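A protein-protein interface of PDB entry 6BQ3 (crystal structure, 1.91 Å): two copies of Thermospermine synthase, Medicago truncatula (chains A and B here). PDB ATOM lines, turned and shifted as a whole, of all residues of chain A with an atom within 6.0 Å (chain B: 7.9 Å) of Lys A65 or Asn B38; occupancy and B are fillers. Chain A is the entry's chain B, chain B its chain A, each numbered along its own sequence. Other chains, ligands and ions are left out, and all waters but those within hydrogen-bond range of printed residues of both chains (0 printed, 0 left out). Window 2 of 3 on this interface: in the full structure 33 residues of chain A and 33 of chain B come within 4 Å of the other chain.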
ATOM      1  N   LYS A  27     -26.687  10.732  34.337  1.00  0.00           N
ATOM      2  CA  LYS A  27     -27.281  10.853  32.956  1.00  0.00           C
ATOM      3  C   LYS A  27     -28.298   9.717  32.679  1.00  0.00           C
ATOM      4  O   LYS A  27     -28.150   8.959  31.719  1.00  0.00           O
ATOM      5  CB  LYS A  27     -26.165  10.883  31.876  1.00  0.00           C
ATOM      6  CG  LYS A  27     -24.970  11.795  32.196  1.00  0.00           C
ATOM      7  CD  LYS A  27     -23.773  11.037  32.801  1.00  0.00           C
ATOM      8  CE  LYS A  27     -23.095  11.767  33.960  1.00  0.00           C
ATOM      9  NZ  LYS A  27     -22.059  12.731  33.497  1.00  0.00           N
ATOM     10  N   TRP A  30     -34.311  11.891  31.589  1.00  0.00           N
ATOM     11  CA  TRP A  30     -34.399  12.459  30.249  1.00  0.00           C
ATOM     12  C   TRP A  30     -35.780  13.019  30.061  1.00  0.00           C
ATOM     13  O   TRP A  30     -36.738  12.416  30.498  1.00  0.00           O
ATOM     14  CB  TRP A  30     -34.178  11.353  29.179  1.00  0.00           C
ATOM     15  CG  TRP A  30     -32.819  10.783  29.212  1.00  0.00           C
ATOM     16  CD1 TRP A  30     -32.404   9.721  29.933  1.00  0.00           C
ATOM     17  CD2 TRP A  30     -31.665  11.284  28.533  1.00  0.00           C
ATOM     18  NE1 TRP A  30     -31.056   9.499  29.739  1.00  0.00           N
ATOM     19  CE2 TRP A  30     -30.580  10.448  28.877  1.00  0.00           C
ATOM     20  CE3 TRP A  30     -31.448  12.334  27.642  1.00  0.00           C
ATOM     21  CZ2 TRP A  30     -29.288  10.642  28.367  1.00  0.00           C
ATOM     22  CZ3 TRP A  30     -30.173  12.520  27.121  1.00  0.00           C
ATOM     23  CH2 TRP A  30     -29.104  11.682  27.497  1.00  0.00           C
ATOM     24  N   CYS A  42     -34.088  13.952  22.883  1.00  0.00           N
ATOM     25  CA  CYS A  42     -34.051  13.768  24.335  1.00  0.00           C
ATOM     26  C   CYS A  42     -32.976  14.633  24.996  1.00  0.00           C
ATOM     27  O   CYS A  42     -31.824  14.675  24.546  1.00  0.00           O
ATOM     28  CB  CYS A  42     -33.816  12.298  24.701  1.00  0.00           C
ATOM     29  SG  CYS A  42     -34.628  11.151  23.563  1.00  0.00           S
ATOM     30  N   PHE A  43     -33.373  15.290  26.084  1.00  0.00           N
ATOM     31  CA  PHE A  43     -32.521  16.212  26.830  1.00  0.00           C
ATOM     32  C   PHE A  43     -32.287  15.642  28.235  1.00  0.00           C
ATOM     33  O   PHE A  43     -33.260  15.369  28.941  1.00  0.00           O
ATOM     34  CB  PHE A  43     -33.260  17.526  27.054  1.00  0.00           C
ATOM     35  CG  PHE A  43     -33.684  18.210  25.831  1.00  0.00           C
ATOM     36  CD1 PHE A  43     -33.061  17.981  24.609  1.00  0.00           C
ATOM     37  CD2 PHE A  43     -34.656  19.183  25.914  1.00  0.00           C
ATOM     38  CE1 PHE A  43     -33.449  18.647  23.480  1.00  0.00           C
ATOM     39  CE2 PHE A  43     -35.060  19.860  24.776  1.00  0.00           C
ATOM     40  CZ  PHE A  43     -34.449  19.612  23.556  1.00  0.00           C
ATOM     41  N   ALA A  44     -31.031  15.476  28.658  1.00  0.00           N
ATOM     42  CA  ALA A  44     -30.776  15.062  30.046  1.00  0.00           C
ATOM     43  C   ALA A  44     -31.418  16.078  31.032  1.00  0.00           C
ATOM     44  O   ALA A  44     -31.342  17.301  30.805  1.00  0.00           O
ATOM     45  CB  ALA A  44     -29.274  14.914  30.311  1.00  0.00           C
ATOM     46  N   LEU A  45     -32.125  15.575  32.049  1.00  0.00           N
ATOM     47  CA  LEU A  45     -32.760  16.449  33.059  1.00  0.00           C
ATOM     48  C   LEU A  45     -31.945  16.595  34.334  1.00  0.00           C
ATOM     49  O   LEU A  45     -31.397  15.611  34.816  1.00  0.00           O
ATOM     50  CB  LEU A  45     -34.082  15.887  33.523  1.00  0.00           C
ATOM     51  CG  LEU A  45     -35.261  15.957  32.629  1.00  0.00           C
ATOM     52  CD1 LEU A  45     -36.337  15.072  33.206  1.00  0.00           C
ATOM     53  CD2 LEU A  45     -35.729  17.393  32.537  1.00  0.00           C
ATOM     54  N   ASN A  46     -31.896  17.808  34.890  1.00  0.00           N
ATOM     55  CA  ASN A  46     -31.467  18.023  36.302  1.00  0.00           C
ATOM     56  C   ASN A  46     -32.644  17.890  37.256  1.00  0.00           C
ATOM     57  O   ASN A  46     -32.514  17.308  38.334  1.00  0.00           O
ATOM     58  CB  ASN A  46     -30.850  19.405  36.509  1.00  0.00           C
ATOM     59  CG  ASN A  46     -29.476  19.540  35.900  1.00  0.00           C
ATOM     60  OD1 ASN A  46     -28.675  18.622  35.967  1.00  0.00           O
ATOM     61  ND2 ASN A  46     -29.206  20.682  35.259  1.00  0.00           N
ATOM     62  N   ASP A  63     -35.564  21.584  34.440  1.00  0.00           N
ATOM     63  CA  ASP A  63     -34.235  22.130  34.430  1.00  0.00           C
ATOM     64  C   ASP A  63     -33.427  21.121  33.649  1.00  0.00           C
ATOM     65  O   ASP A  63     -33.204  20.004  34.141  1.00  0.00           O
ATOM     66  CB  ASP A  63     -33.733  22.312  35.848  1.00  0.00           C
ATOM     67  CG  ASP A  63     -32.373  23.017  35.906  1.00  0.00           C
ATOM     68  OD1 ASP A  63     -31.488  22.757  35.043  1.00  0.00           O
ATOM     69  OD2 ASP A  63     -32.191  23.838  36.792  1.00  0.00           O
ATOM     70  N   THR A  64     -33.045  21.482  32.428  1.00  0.00           N
ATOM     71  CA  THR A  64     -32.349  20.590  31.527  1.00  0.00           C
ATOM     72  C   THR A  64     -30.885  20.899  31.515  1.00  0.00           C
ATOM     73  O   THR A  64     -30.445  22.036  31.758  1.00  0.00           O
ATOM     74  CB  THR A  64     -32.900  20.627  30.102  1.00  0.00           C
ATOM     75  OG1 THR A  64     -32.511  21.825  29.455  1.00  0.00           O
ATOM     76  CG2 THR A  64     -34.459  20.590  30.127  1.00  0.00           C
ATOM     77  N   LYS A  65     -30.127  19.881  31.194  1.00  0.00           N
ATOM     78  CA  LYS A  65     -28.695  20.052  31.116  1.00  0.00           C
ATOM     79  C   LYS A  65     -28.316  20.789  29.887  1.00  0.00           C
ATOM     80  O   LYS A  65     -27.607  21.771  29.990  1.00  0.00           O
ATOM     81  CB  LYS A  65     -27.936  18.724  31.239  1.00  0.00           C
ATOM     82  CG  LYS A  65     -28.145  18.042  32.585  1.00  0.00           C
ATOM     83  CD  LYS A  65     -26.947  17.157  32.953  1.00  0.00           C
ATOM     84  CE  LYS A  65     -27.333  15.892  33.703  1.00  0.00           C
ATOM     85  NZ  LYS A  65     -27.688  16.162  35.116  1.00  0.00           N
ATOM     86  N   PRO A  66     -28.762  20.343  28.703  1.00  0.00           N
ATOM     87  CA  PRO A  66     -28.293  21.135  27.563  1.00  0.00           C
ATOM     88  C   PRO A  66     -28.856  22.565  27.455  1.00  0.00           C
ATOM     89  O   PRO A  66     -28.145  23.446  27.008  1.00  0.00           O
ATOM     90  CB  PRO A  66     -28.687  20.288  26.357  1.00  0.00           C
ATOM     91  CG  PRO A  66     -29.793  19.426  26.860  1.00  0.00           C
ATOM     92  CD  PRO A  66     -29.551  19.169  28.307  1.00  0.00           C
ATOM     93  N   PHE A  67     -30.073  22.832  27.915  1.00  0.00           N
ATOM     94  CA  PHE A  67     -30.681  24.103  27.596  1.00  0.00           C
ATOM     95  C   PHE A  67     -31.146  24.920  28.772  1.00  0.00           C
ATOM     96  O   PHE A  67     -31.833  25.909  28.572  1.00  0.00           O
ATOM     97  CB  PHE A  67     -31.821  23.850  26.599  1.00  0.00           C
ATOM     98  CG  PHE A  67     -31.357  23.189  25.316  1.00  0.00           C
ATOM     99  CD1 PHE A  67     -30.449  23.816  24.515  1.00  0.00           C
ATOM    100  CD2 PHE A  67     -31.805  21.935  24.944  1.00  0.00           C
ATOM    101  CE1 PHE A  67     -30.011  23.236  23.324  1.00  0.00           C
ATOM    102  CE2 PHE A  67     -31.379  21.346  23.758  1.00  0.00           C
ATOM    103  CZ  PHE A  67     -30.477  21.976  22.968  1.00  0.00           C
ATOM    104  N   GLY A  68     -30.738  24.542  29.988  1.00  0.00           N
ATOM    105  CA  GLY A  68     -31.234  25.186  31.217  1.00  0.00           C
ATOM    106  C   GLY A  68     -32.739  24.968  31.435  1.00  0.00           C
ATOM    107  O   GLY A  68     -33.322  23.961  30.992  1.00  0.00           O
ATOM    108  N   GLU B  34     -26.212   9.410  20.472  1.00  0.00           N
ATOM    109  CA  GLU B  34     -25.875  10.369  21.519  1.00  0.00           C
ATOM    110  C   GLU B  34     -25.022  11.355  20.786  1.00  0.00           C
ATOM    111  O   GLU B  34     -23.996  10.996  20.226  1.00  0.00           O
ATOM    112  CB  GLU B  34     -25.126   9.714  22.696  1.00  0.00           C
ATOM    113  CG  GLU B  34     -25.880   8.473  23.229  1.00  0.00           C
ATOM    114  CD  GLU B  34     -25.849   8.274  24.750  1.00  0.00           C
ATOM    115  OE1 GLU B  34     -26.617   8.986  25.478  1.00  0.00           O
ATOM    116  OE2 GLU B  34     -25.102   7.369  25.213  1.00  0.00           O
ATOM    117  N   ILE B  35     -25.493  12.582  20.695  1.00  0.00           N
ATOM    118  CA  ILE B  35     -24.752  13.578  19.933  1.00  0.00           C
ATOM    119  C   ILE B  35     -23.863  14.347  20.898  1.00  0.00           C
ATOM    120  O   ILE B  35     -22.708  14.557  20.606  1.00  0.00           O
ATOM    121  CB  ILE B  35     -25.626  14.416  18.969  1.00  0.00           C
ATOM    122  CG1 ILE B  35     -26.820  15.046  19.654  1.00  0.00           C
ATOM    123  CG2 ILE B  35     -26.099  13.544  17.809  1.00  0.00           C
ATOM    124  CD1 ILE B  35     -27.794  15.679  18.692  1.00  0.00           C
ATOM    125  N   GLU B  36     -24.377  14.704  22.063  1.00  0.00           N
ATOM    126  CA  GLU B  36     -23.537  15.178  23.169  1.00  0.00           C
ATOM    127  C   GLU B  36     -23.785  14.251  24.338  1.00  0.00           C
ATOM    128  O   GLU B  36     -24.705  13.427  24.279  1.00  0.00           O
ATOM    129  CB  GLU B  36     -23.897  16.616  23.561  1.00  0.00           C
ATOM    130  CG  GLU B  36     -23.453  17.688  22.574  1.00  0.00           C
ATOM    131  CD  GLU B  36     -21.954  17.923  22.596  1.00  0.00           C
ATOM    132  OE1 GLU B  36     -21.305  17.712  21.553  1.00  0.00           O
ATOM    133  OE2 GLU B  36     -21.417  18.309  23.667  1.00  0.00           O
ATOM    134  N   GLU B  37     -22.991  14.383  25.410  1.00  0.00           N
ATOM    135  CA  GLU B  37     -23.261  13.579  26.633  1.00  0.00           C
ATOM    136  C   GLU B  37     -24.680  13.813  27.242  1.00  0.00           C
ATOM    137  O   GLU B  37     -25.203  12.901  27.901  1.00  0.00           O
ATOM    138  CB  GLU B  37     -22.141  13.694  27.684  1.00  0.00           C
ATOM    139  CG  GLU B  37     -21.741  15.108  28.096  1.00  0.00           C
ATOM    140  CD  GLU B  37     -20.774  15.139  29.278  1.00  0.00           C
ATOM    141  OE1 GLU B  37     -19.963  14.184  29.431  1.00  0.00           O
ATOM    142  OE2 GLU B  37     -20.817  16.124  30.052  1.00  0.00           O
ATOM    143  N   ASN B  38     -25.313  14.970  26.955  1.00  0.00           N
ATOM    144  CA  ASN B  38     -26.671  15.309  27.455  1.00  0.00           C
ATOM    145  C   ASN B  38     -27.783  15.519  26.399  1.00  0.00           C
ATOM    146  O   ASN B  38     -28.868  16.070  26.694  1.00  0.00           O
ATOM    147  CB  ASN B  38     -26.547  16.567  28.293  1.00  0.00           C
ATOM    148  CG  ASN B  38     -25.613  16.376  29.472  1.00  0.00           C
ATOM    149  OD1 ASN B  38     -24.819  17.255  29.768  1.00  0.00           O
ATOM    150  ND2 ASN B  38     -25.704  15.219  30.140  1.00  0.00           N
ATOM    151  N   LEU B  39     -27.543  15.004  25.203  1.00  0.00           N
ATOM    152  CA  LEU B  39     -28.432  15.175  24.083  1.00  0.00           C
ATOM    153  C   LEU B  39     -28.437  13.896  23.264  1.00  0.00           C
ATOM    154  O   LEU B  39     -27.362  13.486  22.814  1.00  0.00           O
ATOM    155  CB  LEU B  39     -27.883  16.316  23.243  1.00  0.00           C
ATOM    156  CG  LEU B  39     -28.801  17.234  22.477  1.00  0.00           C
ATOM    157  CD1 LEU B  39     -30.098  17.527  23.201  1.00  0.00           C
ATOM    158  CD2 LEU B  39     -28.020  18.524  22.240  1.00  0.00           C
ATOM    159  N   ARG B  40     -29.621  13.298  23.100  1.00  0.00           N
ATOM    160  CA  ARG B  40     -29.860  12.124  22.247  1.00  0.00           C
ATOM    161  C   ARG B  40     -30.944  12.398  21.226  1.00  0.00           C
ATOM    162  O   ARG B  40     -31.917  13.097  21.500  1.00  0.00           O
ATOM    163  CB  ARG B  40     -30.346  10.929  23.059  1.00  0.00           C
ATOM    164  CG  ARG B  40     -29.369  10.520  24.135  1.00  0.00           C
ATOM    165  CD  ARG B  40     -29.734   9.192  24.818  1.00  0.00           C
ATOM    166  NE  ARG B  40     -31.174   8.919  24.918  1.00  0.00           N
ATOM    167  CZ  ARG B  40     -31.700   7.942  25.653  1.00  0.00           C
ATOM    168  NH1 ARG B  40     -30.908   7.145  26.375  1.00  0.00           N
ATOM    169  NH2 ARG B  40     -33.019   7.768  25.682  1.00  0.00           N
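No position is printed for both chains.
Of the 10 pairs that touch across the chains among the printed residues, none has its exchanged pair printed and touching as well.
The backbone NH (N) of Lys A65 is in hydrogen-bond range of the backbone carbonyl oxygen (O) of Ala A44 (2.9 Å).
OD1 of Asn A46 sits at hydrogen-bond distance from NZ of Lys A65, at 2.8 Å.
Of the 13 printed residues of chain A, 6 touch a printed residue of chain B.
Printed residues of chain A that touch a printed residue of chain B: Trp A30, Cys A42, Phe A43, Ala A44, Lys A65 and Pro A66.
Of the 7 printed residues of chain B, 3 touch a printed residue of chain A.
Hydrophobic or aromatic side chains of chain B that line the printed part of chain A: Leu B39.
Among the printed residues, 10 pairs touch across the chains.
Among the printed residues, no Asp or Glu carboxylate lies within 4 Å of a Lys or Arg side-chain nitrogen of the other chain.
Of chain B, only Asn B38 (3.6 Å) comes within 4 Å of Lys A65.
Of chain A, only Trp A30 (3.8 Å), Cys A42 (3.9 Å), Phe A43 (3.7 Å), Ala A44 (3.0 Å), Lys A65 (3.6 Å) and Pro A66 (3.5 Å) come within 4 Å of Asn B38.
Pro A66 touches just one residue of chain B: Asn B38 (3.5 Å).
Of the printed residues of chain B, Phe A43 touches Asn B38 (3.7 Å) and Leu B39 (3.3 Å).
Of the printed residues of chain A, Arg B40 touches Trp A30 (3.6 Å) and Cys A42 (2.7 Å).
Printed residues of chain B within 4 Å of Cys A42: Asn B38 (3.9 Å), Leu B39 (3.5 Å) and Arg B40 (2.7 Å).
Of the printed residues of chain B, Trp A30 touches Asn B38 and Arg B40.
Of the printed residues of chain A, Leu B39 touches Cys A42 and Phe A43.
Gly A68 touches none of the printed residues of chain B.
Asp A63 touches none of the printed residues of chain B.
The nearest residue of chain A that does not touch Asn B38 is Lys A27 (4.1 Å).
Asn B38 touches Trp A30.
Trp A30 touches Arg B40 (CH2 to CG, 3.6 Å).
Asn B38 touches Cys A42.
Leu B39 touches Cys A42 (CA to O, 3.5 Å).
O of Asn B38 touches CA of Phe A43, at 3.7 Å.
Phe A43 touches Leu B39 (CD1 to CD1, 3.3 Å).
CD of Lys A65 touches ND2 of Asn B38, 3.6 Å away.
O of Asn B38 touches CG of Pro A66, 3.5 Å away.
O of Asn B38 sits at hydrogen-bond distance from N of Ala A44 (3.0 Å).
O of Arg B40 sits at hydrogen-bond distance from N of Cys A42.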
